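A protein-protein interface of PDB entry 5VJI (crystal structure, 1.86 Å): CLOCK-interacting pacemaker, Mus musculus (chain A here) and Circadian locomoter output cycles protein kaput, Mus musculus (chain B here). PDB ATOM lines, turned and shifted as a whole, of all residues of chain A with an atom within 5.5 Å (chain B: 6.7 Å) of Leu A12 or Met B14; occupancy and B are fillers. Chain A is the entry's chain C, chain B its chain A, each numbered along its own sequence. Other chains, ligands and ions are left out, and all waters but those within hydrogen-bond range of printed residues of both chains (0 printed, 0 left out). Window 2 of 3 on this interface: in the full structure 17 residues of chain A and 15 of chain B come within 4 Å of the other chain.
The backbone carbonyl oxygen of Val A6 is in hydrogen-bond range of the side-chain hydroxyl of Ser A10 (3.0 Å).
O of Leu A7 lies within hydrogen-bond range of OG of Ser A10 (3.0 Å).
N of Leu A12 lies within hydrogen-bond range of O of Leu A7.
O of Leu A7 sits at hydrogen-bond distance from N of Leu A13, 2.9 Å away.
The side-chain hydroxyl (OG) of Ser A10 sits at hydrogen-bond distance from the backbone NH (N) of Leu A12 (3.2 Å).
O of Leu A12 is in hydrogen-bond range of OG1 of Thr A16, at 2.6 Å.
Among the printed residues, 9 pairs touch across the chains.
Printed residues of chain B within 4 Å of Thr A3: Gln B10 (3.7 Å).
His A8 touches none of the printed residues of chain B.
Of chain B, only Met B14 (3.6 Å) and Leu B21 (3.9 Å) come within 4 Å of Leu A12.
Of the printed residues of chain B, Thr A16 touches Leu B17 (3.7 Å) and Leu B21 (3.6 Å).
Printed residues of chain A within 4 Å of Met B14: Val A6 (3.9 Å), Leu A7 (3.3 Å) and Leu A12 (3.6 Å).
Of the printed residues of chain A, Leu B21 touches Leu A12 (3.9 Å) and Thr A16 (3.6 Å).
The nearest residue of chain B that does not touch Leu A12 is Leu B17 (4.05 Å).
The nearest printed residue of chain B that does not touch Thr A16 is Lys B18 (7.0 Å).
Thr A3 touches Gln B10.
OE1 of Gln B10 touches CG2 of Val A6, 3.5 Å away.
CG of Met B14 touches CG1 of Val A6, at 3.9 Å.
Leu A7 touches Met B14 (CD1 to SD, 3.3 Å).
Leu A7 touches Leu B17 (CD1 to CD2, 3.4 Å).
Met B14 touches Leu A12.
CD1 of Leu B21 touches CD2 of Leu A12 (3.9 Å).
Leu B17 touches Thr A16 (CD2 to OG1, 3.7 Å).
OG1 of Thr A16 touches CD1 of Leu B21, at 3.6 Å.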
ATOM      1  N   THR A   3       7.851   3.498   3.321  1.00  0.00           N
ATOM      2  CA  THR A   3       6.755   4.445   3.111  1.00  0.00           C
ATOM      3  C   THR A   3       5.411   3.861   3.542  1.00  0.00           C
ATOM      4  O   THR A   3       4.584   4.566   4.131  1.00  0.00           O
ATOM      5  CB  THR A   3       6.716   4.873   1.639  1.00  0.00           C
ATOM      6  OG1 THR A   3       7.851   5.711   1.362  1.00  0.00           O
ATOM      7  CG2 THR A   3       5.434   5.633   1.337  1.00  0.00           C
ATOM      8  N   VAL A   6       5.235   4.167   7.279  1.00  0.00           N
ATOM      9  CA  VAL A   6       4.993   5.528   7.752  1.00  0.00           C
ATOM     10  C   VAL A   6       3.552   5.956   7.446  1.00  0.00           C
ATOM     11  O   VAL A   6       2.901   6.639   8.253  1.00  0.00           O
ATOM     12  CB  VAL A   6       6.013   6.474   7.103  1.00  0.00           C
ATOM     13  CG1 VAL A   6       5.590   7.912   7.285  1.00  0.00           C
ATOM     14  CG2 VAL A   6       7.429   6.189   7.648  1.00  0.00           C
ATOM     15  N   LEU A   7       3.021   5.532   6.291  1.00  0.00           N
ATOM     16  CA  LEU A   7       1.637   5.832   5.935  1.00  0.00           C
ATOM     17  C   LEU A   7       0.689   5.249   6.964  1.00  0.00           C
ATOM     18  O   LEU A   7      -0.261   5.904   7.401  1.00  0.00           O
ATOM     19  CB  LEU A   7       1.338   5.240   4.549  1.00  0.00           C
ATOM     20  CG  LEU A   7       0.496   5.816   3.434  1.00  0.00           C
ATOM     21  CD1 LEU A   7       0.604   7.310   3.308  1.00  0.00           C
ATOM     22  CD2 LEU A   7       1.026   5.144   2.152  1.00  0.00           C
ATOM     23  N   HIS A   8       0.954   4.010   7.372  1.00  0.00           N
ATOM     24  CA  HIS A   8       0.134   3.372   8.381  1.00  0.00           C
ATOM     25  C   HIS A   8       0.265   4.077   9.723  1.00  0.00           C
ATOM     26  O   HIS A   8      -0.744   4.446  10.339  1.00  0.00           O
ATOM     27  CB  HIS A   8       0.533   1.894   8.490  1.00  0.00           C
ATOM     28  CG  HIS A   8      -0.279   1.123   9.485  1.00  0.00           C
ATOM     29  ND1 HIS A   8       0.290   0.216  10.361  1.00  0.00           N
ATOM     30  CD2 HIS A   8      -1.621   1.100   9.727  1.00  0.00           C
ATOM     31  CE1 HIS A   8      -0.660  -0.318  11.113  1.00  0.00           C
ATOM     32  NE2 HIS A   8      -1.827   0.205  10.752  1.00  0.00           N
ATOM     33  N   SER A  10       1.264   6.991  10.533  1.00  0.00           N
ATOM     34  CA  SER A  10       0.814   8.378  10.593  1.00  0.00           C
ATOM     35  C   SER A  10      -0.708   8.508  10.655  1.00  0.00           C
ATOM     36  O   SER A  10      -1.203   9.611  10.901  1.00  0.00           O
ATOM     37  CB  SER A  10       1.313   9.137   9.365  1.00  0.00           C
ATOM     38  OG  SER A  10       0.634   8.659   8.232  1.00  0.00           O
ATOM     39  N   GLY A  11      -1.460   7.442  10.416  1.00  0.00           N
ATOM     40  CA  GLY A  11      -2.890   7.565  10.315  1.00  0.00           C
ATOM     41  C   GLY A  11      -3.388   7.841   8.896  1.00  0.00           C
ATOM     42  O   GLY A  11      -4.593   7.681   8.630  1.00  0.00           O
ATOM     43  N   LEU A  12      -2.493   8.204   7.960  1.00  0.00           N
ATOM     44  CA  LEU A  12      -2.956   8.590   6.626  1.00  0.00           C
ATOM     45  C   LEU A  12      -3.334   7.384   5.760  1.00  0.00           C
ATOM     46  O   LEU A  12      -4.112   7.539   4.793  1.00  0.00           O
ATOM     47  CB  LEU A  12      -1.889   9.431   5.901  1.00  0.00           C
ATOM     48  CG  LEU A  12      -1.667  10.774   6.611  1.00  0.00           C
ATOM     49  CD1 LEU A  12      -0.521  11.603   6.084  1.00  0.00           C
ATOM     50  CD2 LEU A  12      -2.986  11.555   6.440  1.00  0.00           C
ATOM     51  N   LEU A  13      -2.779   6.200   6.041  1.00  0.00           N
ATOM     52  CA  LEU A  13      -3.303   5.004   5.359  1.00  0.00           C
ATOM     53  C   LEU A  13      -4.797   4.837   5.635  1.00  0.00           C
ATOM     54  O   LEU A  13      -5.623   4.651   4.728  1.00  0.00           O
ATOM     55  CB  LEU A  13      -2.531   3.753   5.830  1.00  0.00           C
ATOM     56  CG  LEU A  13      -2.956   2.415   5.162  1.00  0.00           C
ATOM     57  CD1 LEU A  13      -2.938   2.486   3.665  1.00  0.00           C
ATOM     58  CD2 LEU A  13      -2.078   1.244   5.682  1.00  0.00           C
ATOM     59  N   GLU A  14      -5.163   4.879   6.898  1.00  0.00           N
ATOM     60  CA  GLU A  14      -6.558   4.700   7.253  1.00  0.00           C
ATOM     61  C   GLU A  14      -7.408   5.786   6.633  1.00  0.00           C
ATOM     62  O   GLU A  14      -8.449   5.513   6.018  1.00  0.00           O
ATOM     63  CB  GLU A  14      -6.716   4.730   8.757  1.00  0.00           C
ATOM     64  CG  GLU A  14      -8.222   4.741   9.161  1.00  0.00           C
ATOM     65  CD  GLU A  14      -8.442   4.779  10.679  1.00  0.00           C
ATOM     66  OE1 GLU A  14      -7.625   4.184  11.422  1.00  0.00           O
ATOM     67  OE2 GLU A  14      -9.437   5.416  11.126  1.00  0.00           O
ATOM     68  N   ILE A  15      -6.976   7.026   6.750  1.00  0.00           N
ATOM     69  CA  ILE A  15      -7.786   8.121   6.203  1.00  0.00           C
ATOM     70  C   ILE A  15      -7.888   8.042   4.694  1.00  0.00           C
ATOM     71  O   ILE A  15      -8.944   8.372   4.120  1.00  0.00           O
ATOM     72  CB  ILE A  15      -7.230   9.483   6.618  1.00  0.00           C
ATOM     73  CG1 ILE A  15      -7.291   9.618   8.140  1.00  0.00           C
ATOM     74  CG2 ILE A  15      -8.068  10.591   5.973  1.00  0.00           C
ATOM     75  CD1 ILE A  15      -6.507  10.835   8.723  1.00  0.00           C
ATOM     76  N   THR A  16      -6.783   7.708   4.015  1.00  0.00           N
ATOM     77  CA  THR A  16      -6.830   7.624   2.551  1.00  0.00           C
ATOM     78  C   THR A  16      -7.798   6.540   2.118  1.00  0.00           C
ATOM     79  O   THR A  16      -8.555   6.719   1.155  1.00  0.00           O
ATOM     80  CB  THR A  16      -5.445   7.323   1.940  1.00  0.00           C
ATOM     81  OG1 THR A  16      -4.505   8.318   2.343  1.00  0.00           O
ATOM     82  CG2 THR A  16      -5.520   7.389   0.408  1.00  0.00           C
ATOM     83  N   LEU A  17      -7.788   5.404   2.812  1.00  0.00           N
ATOM     84  CA  LEU A  17      -8.713   4.321   2.491  1.00  0.00           C
ATOM     85  C   LEU A  17     -10.168   4.745   2.716  1.00  0.00           C
ATOM     86  O   LEU A  17     -11.050   4.438   1.904  1.00  0.00           O
ATOM     87  CB  LEU A  17      -8.363   3.073   3.336  1.00  0.00           C
ATOM     88  CG  LEU A  17      -7.029   2.395   2.995  1.00  0.00           C
ATOM     89  CD1 LEU A  17      -6.830   1.233   3.942  1.00  0.00           C
ATOM     90  CD2 LEU A  17      -6.978   1.932   1.553  1.00  0.00           C
ATOM     91  N   ALA B   9      12.131  13.086   3.125  1.00  0.00           N
ATOM     92  CA  ALA B   9      11.215  13.036   1.984  1.00  0.00           C
ATOM     93  C   ALA B   9       9.860  12.496   2.407  1.00  0.00           C
ATOM     94  O   ALA B   9       8.810  12.899   1.869  1.00  0.00           O
ATOM     95  CB  ALA B   9      11.786  12.173   0.875  1.00  0.00           C
ATOM     96  N   GLN B  10       9.870  11.537   3.329  1.00  0.00           N
ATOM     97  CA  GLN B  10       8.606  10.978   3.803  1.00  0.00           C
ATOM     98  C   GLN B  10       7.800  12.045   4.526  1.00  0.00           C
ATOM     99  O   GLN B  10       6.563  12.081   4.437  1.00  0.00           O
ATOM    100  CB  GLN B  10       8.876   9.776   4.728  1.00  0.00           C
ATOM    101  CG  GLN B  10       9.370   8.533   3.975  1.00  0.00           C
ATOM    102  CD  GLN B  10       9.924   7.428   4.883  1.00  0.00           C
ATOM    103  OE1 GLN B  10      10.197   7.644   6.069  1.00  0.00           O
ATOM    104  NE2 GLN B  10      10.107   6.240   4.313  1.00  0.00           N
ATOM    105  N   LEU B  11       8.483  12.904   5.278  1.00  0.00           N
ATOM    106  CA  LEU B  11       7.832  14.043   5.931  1.00  0.00           C
ATOM    107  C   LEU B  11       7.097  14.933   4.918  1.00  0.00           C
ATOM    108  O   LEU B  11       5.916  15.282   5.100  1.00  0.00           O
ATOM    109  CB  LEU B  11       8.913  14.832   6.673  1.00  0.00           C
ATOM    110  CG  LEU B  11       8.614  16.091   7.467  1.00  0.00           C
ATOM    111  CD1 LEU B  11       7.441  15.834   8.406  1.00  0.00           C
ATOM    112  CD2 LEU B  11       9.874  16.466   8.244  1.00  0.00           C
ATOM    113  N   GLY B  12       7.779  15.318   3.831  1.00  0.00           N
ATOM    114  CA  GLY B  12       7.137  16.155   2.828  1.00  0.00           C
ATOM    115  C   GLY B  12       6.047  15.421   2.066  1.00  0.00           C
ATOM    116  O   GLY B  12       5.010  16.003   1.715  1.00  0.00           O
ATOM    117  N   ALA B  13       6.258  14.134   1.806  1.00  0.00           N
ATOM    118  CA  ALA B  13       5.237  13.322   1.151  1.00  0.00           C
ATOM    119  C   ALA B  13       3.972  13.188   1.996  1.00  0.00           C
ATOM    120  O   ALA B  13       2.868  13.240   1.451  1.00  0.00           O
ATOM    121  CB  ALA B  13       5.789  11.929   0.826  1.00  0.00           C
ATOM    122  N   MET B  14       4.100  12.951   3.312  1.00  0.00           N
ATOM    123  CA  MET B  14       2.888  12.862   4.145  1.00  0.00           C
ATOM    124  C   MET B  14       2.178  14.226   4.253  1.00  0.00           C
ATOM    125  O   MET B  14       0.965  14.272   4.225  1.00  0.00           O
ATOM    126  CB  MET B  14       3.197  12.344   5.567  1.00  0.00           C
ATOM    127  CG  MET B  14       3.766  10.913   5.613  1.00  0.00           C
ATOM    128  SD  MET B  14       2.634   9.561   4.679  1.00  0.00           S
ATOM    129  CE  MET B  14       3.524   9.516   2.915  1.00  0.00           C
ATOM    130  N   GLN B  15       2.909  15.342   4.418  1.00  0.00           N
ATOM    131  CA  GLN B  15       2.271  16.656   4.433  1.00  0.00           C
ATOM    132  C   GLN B  15       1.504  16.907   3.137  1.00  0.00           C
ATOM    133  O   GLN B  15       0.374  17.418   3.152  1.00  0.00           O
ATOM    134  CB  GLN B  15       3.346  17.728   4.688  1.00  0.00           C
ATOM    135  CG  GLN B  15       3.989  17.558   6.077  1.00  0.00           C
ATOM    136  CD  GLN B  15       5.125  18.550   6.411  1.00  0.00           C
ATOM    137  OE1 GLN B  15       6.291  18.233   6.255  1.00  0.00           O
ATOM    138  NE2 GLN B  15       4.767  19.724   6.920  1.00  0.00           N
ATOM    139  N   HIS B  16       2.108  16.539   2.001  1.00  0.00           N
ATOM    140  CA  HIS B  16       1.445  16.696   0.713  1.00  0.00           C
ATOM    141  C   HIS B  16       0.178  15.857   0.640  1.00  0.00           C
ATOM    142  O   HIS B  16      -0.870  16.336   0.174  1.00  0.00           O
ATOM    143  CB  HIS B  16       2.378  16.305  -0.435  1.00  0.00           C
ATOM    144  CG  HIS B  16       1.735  16.411  -1.773  1.00  0.00           C
ATOM    145  ND1 HIS B  16       1.626  17.608  -2.450  1.00  0.00           N
ATOM    146  CD2 HIS B  16       1.116  15.482  -2.541  1.00  0.00           C
ATOM    147  CE1 HIS B  16       0.982  17.409  -3.587  1.00  0.00           C
ATOM    148  NE2 HIS B  16       0.659  16.129  -3.665  1.00  0.00           N
ATOM    149  N   LEU B  17       0.266  14.604   1.070  1.00  0.00           N
ATOM    150  CA  LEU B  17      -0.889  13.710   1.031  1.00  0.00           C
ATOM    151  C   LEU B  17      -1.981  14.217   1.943  1.00  0.00           C
ATOM    152  O   LEU B  17      -3.161  14.137   1.596  1.00  0.00           O
ATOM    153  CB  LEU B  17      -0.492  12.290   1.460  1.00  0.00           C
ATOM    154  CG  LEU B  17      -1.655  11.292   1.571  1.00  0.00           C
ATOM    155  CD1 LEU B  17      -2.361  11.217   0.259  1.00  0.00           C
ATOM    156  CD2 LEU B  17      -1.136   9.898   1.953  1.00  0.00           C
ATOM    157  N   LYS B  18      -1.621  14.672   3.150  1.00  0.00           N
ATOM    158  CA  LYS B  18      -2.631  15.287   4.022  1.00  0.00           C
ATOM    159  C   LYS B  18      -3.359  16.435   3.316  1.00  0.00           C
ATOM    160  O   LYS B  18      -4.599  16.543   3.389  1.00  0.00           O
ATOM    161  CB  LYS B  18      -1.973  15.772   5.309  1.00  0.00           C
ATOM    162  CG  LYS B  18      -2.968  16.390   6.238  1.00  0.00           C
ATOM    163  CD  LYS B  18      -2.445  16.406   7.645  1.00  0.00           C
ATOM    164  CE  LYS B  18      -3.578  16.634   8.653  1.00  0.00           C
ATOM    165  NZ  LYS B  18      -3.946  18.064   8.761  1.00  0.00           N
ATOM    166  N   ASP B  19      -2.600  17.342   2.671  1.00  0.00           N
ATOM    167  CA  ASP B  19      -3.214  18.449   1.922  1.00  0.00           C
ATOM    168  C   ASP B  19      -4.141  17.944   0.814  1.00  0.00           C
ATOM    169  O   ASP B  19      -5.251  18.458   0.635  1.00  0.00           O
ATOM    170  CB  ASP B  19      -2.126  19.351   1.337  1.00  0.00           C
ATOM    171  CG  ASP B  19      -1.287  20.045   2.412  1.00  0.00           C
ATOM    172  OD1 ASP B  19      -1.621  19.958   3.615  1.00  0.00           O
ATOM    173  OD2 ASP B  19      -0.284  20.691   2.051  1.00  0.00           O
ATOM    174  N   LEU B  21      -5.729  15.033   0.695  1.00  0.00           N
ATOM    175  CA  LEU B  21      -6.927  14.483   1.350  1.00  0.00           C
ATOM    176  C   LEU B  21      -7.877  15.564   1.854  1.00  0.00           C
ATOM    177  O   LEU B  21      -9.101  15.438   1.698  1.00  0.00           O
ATOM    178  CB  LEU B  21      -6.522  13.599   2.514  1.00  0.00           C
ATOM    179  CG  LEU B  21      -5.811  12.348   2.051  1.00  0.00           C
ATOM    180  CD1 LEU B  21      -5.249  11.726   3.300  1.00  0.00           C
ATOM    181  CD2 LEU B  21      -6.802  11.407   1.419  1.00  0.00           C
